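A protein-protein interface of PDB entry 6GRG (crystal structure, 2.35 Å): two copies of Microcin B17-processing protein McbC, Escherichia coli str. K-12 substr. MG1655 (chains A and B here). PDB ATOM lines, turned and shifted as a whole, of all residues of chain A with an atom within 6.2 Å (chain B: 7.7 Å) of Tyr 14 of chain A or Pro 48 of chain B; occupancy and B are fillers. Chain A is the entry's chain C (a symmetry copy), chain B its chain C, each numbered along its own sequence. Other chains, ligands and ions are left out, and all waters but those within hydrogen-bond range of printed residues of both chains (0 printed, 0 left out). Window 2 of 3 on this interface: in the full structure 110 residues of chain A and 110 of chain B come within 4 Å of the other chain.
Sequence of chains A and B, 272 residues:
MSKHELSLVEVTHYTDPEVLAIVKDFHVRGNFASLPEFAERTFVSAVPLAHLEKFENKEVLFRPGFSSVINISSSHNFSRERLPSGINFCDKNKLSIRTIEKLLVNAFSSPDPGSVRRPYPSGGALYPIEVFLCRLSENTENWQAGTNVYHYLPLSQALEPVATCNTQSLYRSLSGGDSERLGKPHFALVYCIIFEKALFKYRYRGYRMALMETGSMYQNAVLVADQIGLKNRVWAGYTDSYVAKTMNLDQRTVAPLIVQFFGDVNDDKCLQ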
ATOM      1  N   GLU A  10      25.689  16.702  13.707  1.00  0.00           N
ATOM      2  CA  GLU A  10      24.877  17.512  14.611  1.00  0.00           C
ATOM      3  C   GLU A  10      24.412  18.780  13.890  1.00  0.00           C
ATOM      4  O   GLU A  10      23.293  19.215  14.046  1.00  0.00           O
ATOM      5  CB  GLU A  10      25.681  17.871  15.860  1.00  0.00           C
ATOM      6  CG  GLU A  10      26.025  16.671  16.717  1.00  0.00           C
ATOM      7  CD  GLU A  10      24.895  16.156  17.590  1.00  0.00           C
ATOM      8  OE1 GLU A  10      23.889  16.862  17.729  1.00  0.00           O
ATOM      9  OE2 GLU A  10      25.037  15.057  18.154  1.00  0.00           O
ATOM     10  N   VAL A  11      25.318  19.349  13.098  1.00  0.00           N
ATOM     11  CA  VAL A  11      25.115  20.567  12.374  1.00  0.00           C
ATOM     12  C   VAL A  11      24.008  20.381  11.325  1.00  0.00           C
ATOM     13  O   VAL A  11      23.098  21.199  11.235  1.00  0.00           O
ATOM     14  CB  VAL A  11      26.428  21.046  11.722  1.00  0.00           C
ATOM     15  CG1 VAL A  11      26.185  22.187  10.753  1.00  0.00           C
ATOM     16  CG2 VAL A  11      27.452  21.428  12.781  1.00  0.00           C
ATOM     17  N   THR A  12      24.087  19.310  10.543  1.00  0.00           N
ATOM     18  CA  THR A  12      23.203  19.158   9.393  1.00  0.00           C
ATOM     19  C   THR A  12      21.742  19.010   9.836  1.00  0.00           C
ATOM     20  O   THR A  12      20.867  19.258   9.024  1.00  0.00           O
ATOM     21  CB  THR A  12      23.609  17.999   8.472  1.00  0.00           C
ATOM     22  OG1 THR A  12      22.958  18.244   7.224  1.00  0.00           O
ATOM     23  CG2 THR A  12      23.268  16.615   9.002  1.00  0.00           C
ATOM     24  N   HIS A  13      21.488  18.659  11.106  1.00  0.00           N
ATOM     25  CA  HIS A  13      20.130  18.491  11.614  1.00  0.00           C
ATOM     26  C   HIS A  13      19.350  19.820  11.516  1.00  0.00           C
ATOM     27  O   HIS A  13      18.119  19.831  11.552  1.00  0.00           O
ATOM     28  CB  HIS A  13      20.214  17.873  13.016  1.00  0.00           C
ATOM     29  CG  HIS A  13      18.931  17.730  13.760  1.00  0.00           C
ATOM     30  ND1 HIS A  13      18.076  16.657  13.568  1.00  0.00           N
ATOM     31  CD2 HIS A  13      18.392  18.471  14.762  1.00  0.00           C
ATOM     32  CE1 HIS A  13      17.044  16.766  14.392  1.00  0.00           C
ATOM     33  NE2 HIS A  13      17.219  17.872  15.141  1.00  0.00           N
ATOM     34  N   TYR A  14      20.063  20.940  11.366  1.00  0.00           N
ATOM     35  CA  TYR A  14      19.443  22.246  11.317  1.00  0.00           C
ATOM     36  C   TYR A  14      19.540  22.878   9.926  1.00  0.00           C
ATOM     37  O   TYR A  14      19.166  24.016   9.782  1.00  0.00           O
ATOM     38  CB  TYR A  14      20.109  23.186  12.329  1.00  0.00           C
ATOM     39  CG  TYR A  14      19.901  22.757  13.758  1.00  0.00           C
ATOM     40  CD1 TYR A  14      18.687  22.958  14.393  1.00  0.00           C
ATOM     41  CD2 TYR A  14      20.895  22.091  14.459  1.00  0.00           C
ATOM     42  CE1 TYR A  14      18.469  22.506  15.688  1.00  0.00           C
ATOM     43  CE2 TYR A  14      20.696  21.642  15.752  1.00  0.00           C
ATOM     44  CZ  TYR A  14      19.480  21.856  16.372  1.00  0.00           C
ATOM     45  OH  TYR A  14      19.300  21.440  17.661  1.00  0.00           O
ATOM     46  N   THR A  15      20.094  22.190   8.927  1.00  0.00           N
ATOM     47  CA  THR A  15      20.340  22.807   7.625  1.00  0.00           C
ATOM     48  C   THR A  15      19.009  23.004   6.879  1.00  0.00           C
ATOM     49  O   THR A  15      18.174  22.107   6.763  1.00  0.00           O
ATOM     50  CB  THR A  15      21.354  22.003   6.793  1.00  0.00           C
ATOM     51  OG1 THR A  15      22.637  22.230   7.365  1.00  0.00           O
ATOM     52  CG2 THR A  15      21.396  22.379   5.322  1.00  0.00           C
ATOM     53  N   ASP A  16      18.809  24.232   6.394  1.00  0.00           N
ATOM     54  CA  ASP A  16      17.816  24.517   5.394  1.00  0.00           C
ATOM     55  C   ASP A  16      18.446  24.199   4.035  1.00  0.00           C
ATOM     56  O   ASP A  16      19.407  24.836   3.589  1.00  0.00           O
ATOM     57  CB  ASP A  16      17.299  25.947   5.550  1.00  0.00           C
ATOM     58  CG  ASP A  16      16.179  26.257   4.579  1.00  0.00           C
ATOM     59  OD1 ASP A  16      16.006  25.499   3.580  1.00  0.00           O
ATOM     60  OD2 ASP A  16      15.469  27.228   4.840  1.00  0.00           O
ATOM     61  N   LEU A 199      26.051  28.242   7.742  1.00  0.00           N
ATOM     62  CA  LEU A 199      24.647  28.557   7.393  1.00  0.00           C
ATOM     63  C   LEU A 199      23.637  28.116   8.453  1.00  0.00           C
ATOM     64  O   LEU A 199      22.580  28.731   8.539  1.00  0.00           O
ATOM     65  CB  LEU A 199      24.314  27.911   6.047  1.00  0.00           C
ATOM     66  CG  LEU A 199      25.030  28.544   4.851  1.00  0.00           C
ATOM     67  CD1 LEU A 199      24.630  27.845   3.567  1.00  0.00           C
ATOM     68  CD2 LEU A 199      24.743  30.035   4.752  1.00  0.00           C
ATOM     69  N   PHE A 200      23.944  27.086   9.257  1.00  0.00           N
ATOM     70  CA  PHE A 200      22.899  26.391  10.020  1.00  0.00           C
ATOM     71  C   PHE A 200      22.180  27.293  11.037  1.00  0.00           C
ATOM     72  O   PHE A 200      20.965  27.099  11.264  1.00  0.00           O
ATOM     73  CB  PHE A 200      23.433  25.119  10.685  1.00  0.00           C
ATOM     74  CG  PHE A 200      24.237  25.264  11.955  1.00  0.00           C
ATOM     75  CD1 PHE A 200      25.438  25.946  11.969  1.00  0.00           C
ATOM     76  CD2 PHE A 200      23.848  24.600  13.110  1.00  0.00           C
ATOM     77  CE1 PHE A 200      26.203  26.003  13.121  1.00  0.00           C
ATOM     78  CE2 PHE A 200      24.614  24.662  14.259  1.00  0.00           C
ATOM     79  CZ  PHE A 200      25.784  25.381  14.268  1.00  0.00           C
ATOM     80  N   LYS A 201      22.905  28.234  11.659  1.00  0.00           N
ATOM     81  CA  LYS A 201      22.333  29.053  12.733  1.00  0.00           C
ATOM     82  C   LYS A 201      21.666  30.338  12.199  1.00  0.00           C
ATOM     83  O   LYS A 201      20.523  30.651  12.551  1.00  0.00           O
ATOM     84  CB  LYS A 201      23.394  29.401  13.779  1.00  0.00           C
ATOM     85  CG  LYS A 201      22.844  30.230  14.920  1.00  0.00           C
ATOM     86  CD  LYS A 201      23.751  30.374  16.102  1.00  0.00           C
ATOM     87  CE  LYS A 201      23.014  31.062  17.233  1.00  0.00           C
ATOM     88  NZ  LYS A 201      23.883  32.009  17.960  1.00  0.00           N
ATOM     89  N   SER B  45      17.996  32.655  15.461  1.00  0.00           N
ATOM     90  CA  SER B  45      18.755  31.398  15.513  1.00  0.00           C
ATOM     91  C   SER B  45      17.861  30.248  15.052  1.00  0.00           C
ATOM     92  O   SER B  45      16.771  30.102  15.581  1.00  0.00           O
ATOM     93  CB  SER B  45      19.283  31.163  16.917  1.00  0.00           C
ATOM     94  OG  SER B  45      19.950  29.911  17.047  1.00  0.00           O
ATOM     95  N   ALA B  46      18.322  29.433  14.091  1.00  0.00           N
ATOM     96  CA  ALA B  46      17.575  28.227  13.733  1.00  0.00           C
ATOM     97  C   ALA B  46      17.820  27.148  14.790  1.00  0.00           C
ATOM     98  O   ALA B  46      17.038  26.247  14.924  1.00  0.00           O
ATOM     99  CB  ALA B  46      17.931  27.756  12.350  1.00  0.00           C
ATOM    100  N   VAL B  47      18.873  27.301  15.594  1.00  0.00           N
ATOM    101  CA  VAL B  47      19.147  26.394  16.694  1.00  0.00           C
ATOM    102  C   VAL B  47      18.563  26.925  18.002  1.00  0.00           C
ATOM    103  O   VAL B  47      18.919  28.008  18.437  1.00  0.00           O
ATOM    104  CB  VAL B  47      20.660  26.193  16.855  1.00  0.00           C
ATOM    105  CG1 VAL B  47      20.933  25.116  17.901  1.00  0.00           C
ATOM    106  CG2 VAL B  47      21.337  25.892  15.521  1.00  0.00           C
ATOM    107  N   PRO B  48      17.727  26.143  18.714  1.00  0.00           N
ATOM    108  CA  PRO B  48      17.329  26.463  20.093  1.00  0.00           C
ATOM    109  C   PRO B  48      18.483  26.813  21.049  1.00  0.00           C
ATOM    110  O   PRO B  48      19.535  26.229  20.947  1.00  0.00           O
ATOM    111  CB  PRO B  48      16.686  25.149  20.571  1.00  0.00           C
ATOM    112  CG  PRO B  48      16.108  24.539  19.305  1.00  0.00           C
ATOM    113  CD  PRO B  48      17.118  24.895  18.227  1.00  0.00           C
ATOM    114  N   LEU B  49      18.247  27.752  21.972  1.00  0.00           N
ATOM    115  CA  LEU B  49      19.243  28.255  22.951  1.00  0.00           C
ATOM    116  C   LEU B  49      19.891  27.089  23.701  1.00  0.00           C
ATOM    117  O   LEU B  49      21.090  27.125  24.003  1.00  0.00           O
ATOM    118  CB  LEU B  49      18.561  29.187  23.962  1.00  0.00           C
ATOM    119  N   ALA B  50      19.074  26.076  24.004  1.00  0.00           N
ATOM    120  CA  ALA B  50      19.447  24.955  24.841  1.00  0.00           C
ATOM    121  C   ALA B  50      20.377  23.974  24.125  1.00  0.00           C
ATOM    122  O   ALA B  50      20.916  23.132  24.777  1.00  0.00           O
ATOM    123  CB  ALA B  50      18.201  24.237  25.279  1.00  0.00           C
ATOM    124  N   HIS B  51      20.504  24.039  22.795  1.00  0.00           N
ATOM    125  CA  HIS B  51      21.352  23.086  22.065  1.00  0.00           C
ATOM    126  C   HIS B  51      22.607  23.778  21.533  1.00  0.00           C
ATOM    127  O   HIS B  51      23.456  23.123  20.951  1.00  0.00           O
ATOM    128  CB  HIS B  51      20.573  22.398  20.938  1.00  0.00           C
ATOM    129  CG  HIS B  51      19.594  21.358  21.397  1.00  0.00           C
ATOM    130  ND1 HIS B  51      19.989  20.118  21.890  1.00  0.00           N
ATOM    131  CD2 HIS B  51      18.242  21.347  21.418  1.00  0.00           C
ATOM    132  CE1 HIS B  51      18.924  19.402  22.203  1.00  0.00           C
ATOM    133  NE2 HIS B  51      17.842  20.135  21.920  1.00  0.00           N
ATOM    134  N   LEU B  52      22.731  25.087  21.778  1.00  0.00           N
ATOM    135  CA  LEU B  52      23.736  25.929  21.137  1.00  0.00           C
ATOM    136  C   LEU B  52      25.146  25.620  21.654  1.00  0.00           C
ATOM    137  O   LEU B  52      26.088  25.633  20.896  1.00  0.00           O
ATOM    138  CB  LEU B  52      23.404  27.409  21.372  1.00  0.00           C
ATOM    139  CG  LEU B  52      22.583  28.123  20.289  1.00  0.00           C
ATOM    140  CD1 LEU B  52      22.301  29.560  20.693  1.00  0.00           C
ATOM    141  CD2 LEU B  52      23.280  28.121  18.939  1.00  0.00           C
ATOM    142  N   GLU B  53      25.293  25.368  22.953  1.00  0.00           N
ATOM    143  CA  GLU B  53      26.612  25.284  23.591  1.00  0.00           C
ATOM    144  C   GLU B  53      27.460  24.179  22.928  1.00  0.00           C
ATOM    145  O   GLU B  53      28.690  24.304  22.770  1.00  0.00           O
ATOM    146  CB  GLU B  53      26.374  25.111  25.095  1.00  0.00           C
ATOM    147  CG  GLU B  53      27.630  25.049  25.937  1.00  0.00           C
ATOM    148  CD  GLU B  53      27.934  23.651  26.433  1.00  0.00           C
ATOM    149  OE1 GLU B  53      27.781  23.413  27.655  1.00  0.00           O
ATOM    150  OE2 GLU B  53      28.307  22.800  25.592  1.00  0.00           O
ATOM    151  N   LYS B  54      26.781  23.107  22.505  1.00  0.00           N
ATOM    152  CA  LYS B  54      27.359  21.961  21.812  1.00  0.00           C
ATOM    153  C   LYS B  54      28.005  22.404  20.489  1.00  0.00           C
ATOM    154  O   LYS B  54      28.821  21.683  19.931  1.00  0.00           O
ATOM    155  CB  LYS B  54      26.239  20.922  21.645  1.00  0.00           C
ATOM    156  CG  LYS B  54      26.364  19.914  20.503  1.00  0.00           C
ATOM    157  CD  LYS B  54      25.098  19.764  19.669  1.00  0.00           C
ATOM    158  CE  LYS B  54      23.892  19.299  20.461  1.00  0.00           C
ATOM    159  NZ  LYS B  54      22.631  19.692  19.789  1.00  0.00           N
ATOM    160  N   PHE B  55      27.644  23.584  19.972  1.00  0.00           N
ATOM    161  CA  PHE B  55      28.146  24.017  18.679  1.00  0.00           C
ATOM    162  C   PHE B  55      29.192  25.129  18.820  1.00  0.00           C
ATOM    163  O   PHE B  55      29.809  25.509  17.831  1.00  0.00           O
ATOM    164  CB  PHE B  55      26.989  24.474  17.791  1.00  0.00           C
ATOM    165  CG  PHE B  55      25.979  23.412  17.429  1.00  0.00           C
ATOM    166  CD1 PHE B  55      26.261  22.456  16.457  1.00  0.00           C
ATOM    167  CD2 PHE B  55      24.722  23.391  18.018  1.00  0.00           C
ATOM    168  CE1 PHE B  55      25.322  21.492  16.105  1.00  0.00           C
ATOM    169  CE2 PHE B  55      23.776  22.434  17.653  1.00  0.00           C
ATOM    170  CZ  PHE B  55      24.086  21.469  16.718  1.00  0.00           C
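The backbone carbonyl oxygen of Lys 201 of chain A lies within hydrogen-bond range of the backbone NH of Ala 46 of chain B (2.9 Å). The side-chain amino group (NZ) of Lys 54 of chain B lies within salt-bridge range of the side-chain carboxylate (OE1) of Glu 10 of chain A, at 3.7 Å.
O of Val 47 of chain B is in hydrogen-bond range of OG of Ser 45 of chain B (2.6 Å). A ring nitrogen (ND1) of His 51 of chain B is in hydrogen-bond range of the side-chain amino group (NZ) of Lys 54 of chain B (3.4 Å).
Glu 10 of chain A touches Phe 55 of chain B. CE1 of Phe 55 of chain B touches N of Val 11 of chain A, at 3.7 Å. Tyr 14 of chain A touches Ala 46 of chain B (CD1 to O, 3.7 Å). Tyr 14 of chain A touches Val 47 of chain B. Tyr 14 of chain A touches Pro 48 of chain B. Phe 200 of chain A touches Ala 46 of chain B. CD2 of Phe 200 of chain A touches CG2 of Val 47 of chain B, 3.7 Å away. Phe 200 of chain A touches Phe 55 of chain B. Lys 201 of chain A touches Ser 45 of chain B (CE to OG, 3.3 Å). CE of Lys 201 of chain A touches CD2 of Leu 52 of chain B (3.4 Å).
Of chain B, only Ala 46, Val 47, Pro 48, His 51 and Phe 55 come within 4 Å of Tyr 14 of chain A. Pro 48 of chain B touches just one residue of chain A: Tyr 14 (3.7 Å). Of the printed residues of chain B, Glu 10 of chain A touches Lys 54 and Phe 55. Of the printed residues of chain A, Lys 54 of chain B touches Glu 10. Printed residues of chain A within 4 Å of Val 47 of chain B: Tyr 14 (3.9 Å) and Phe 200 (3.7 Å). Of the printed residues of chain A, Phe 55 of chain B touches Glu 10 (3.6 Å), Val 11 (3.7 Å), Tyr 14 (3.5 Å) and Phe 200 (3.5 Å). The nearest residue of chain B that does not touch Tyr 14 of chain A is Lys 54 of chain B (4.3 Å). The nearest printed residue of chain A that does not touch Pro 48 of chain B is Lys 201 of chain A (7.0 Å). The nearest printed residue of chain B that does not touch Val 11 of chain A is Lys 54 of chain B (6.6 Å).
Hydrophobic or aromatic side chains of chain A that line the printed part of chain B: Val 11, Tyr 14 and Phe 200. Hydrophobic or aromatic side chains of chain B that line the printed part of chain A: Ala 46, Val 47, Pro 48, His 51, Leu 52 and Phe 55. Among the printed residues, 14 pairs touch across the chains.
No position is printed for both chains.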
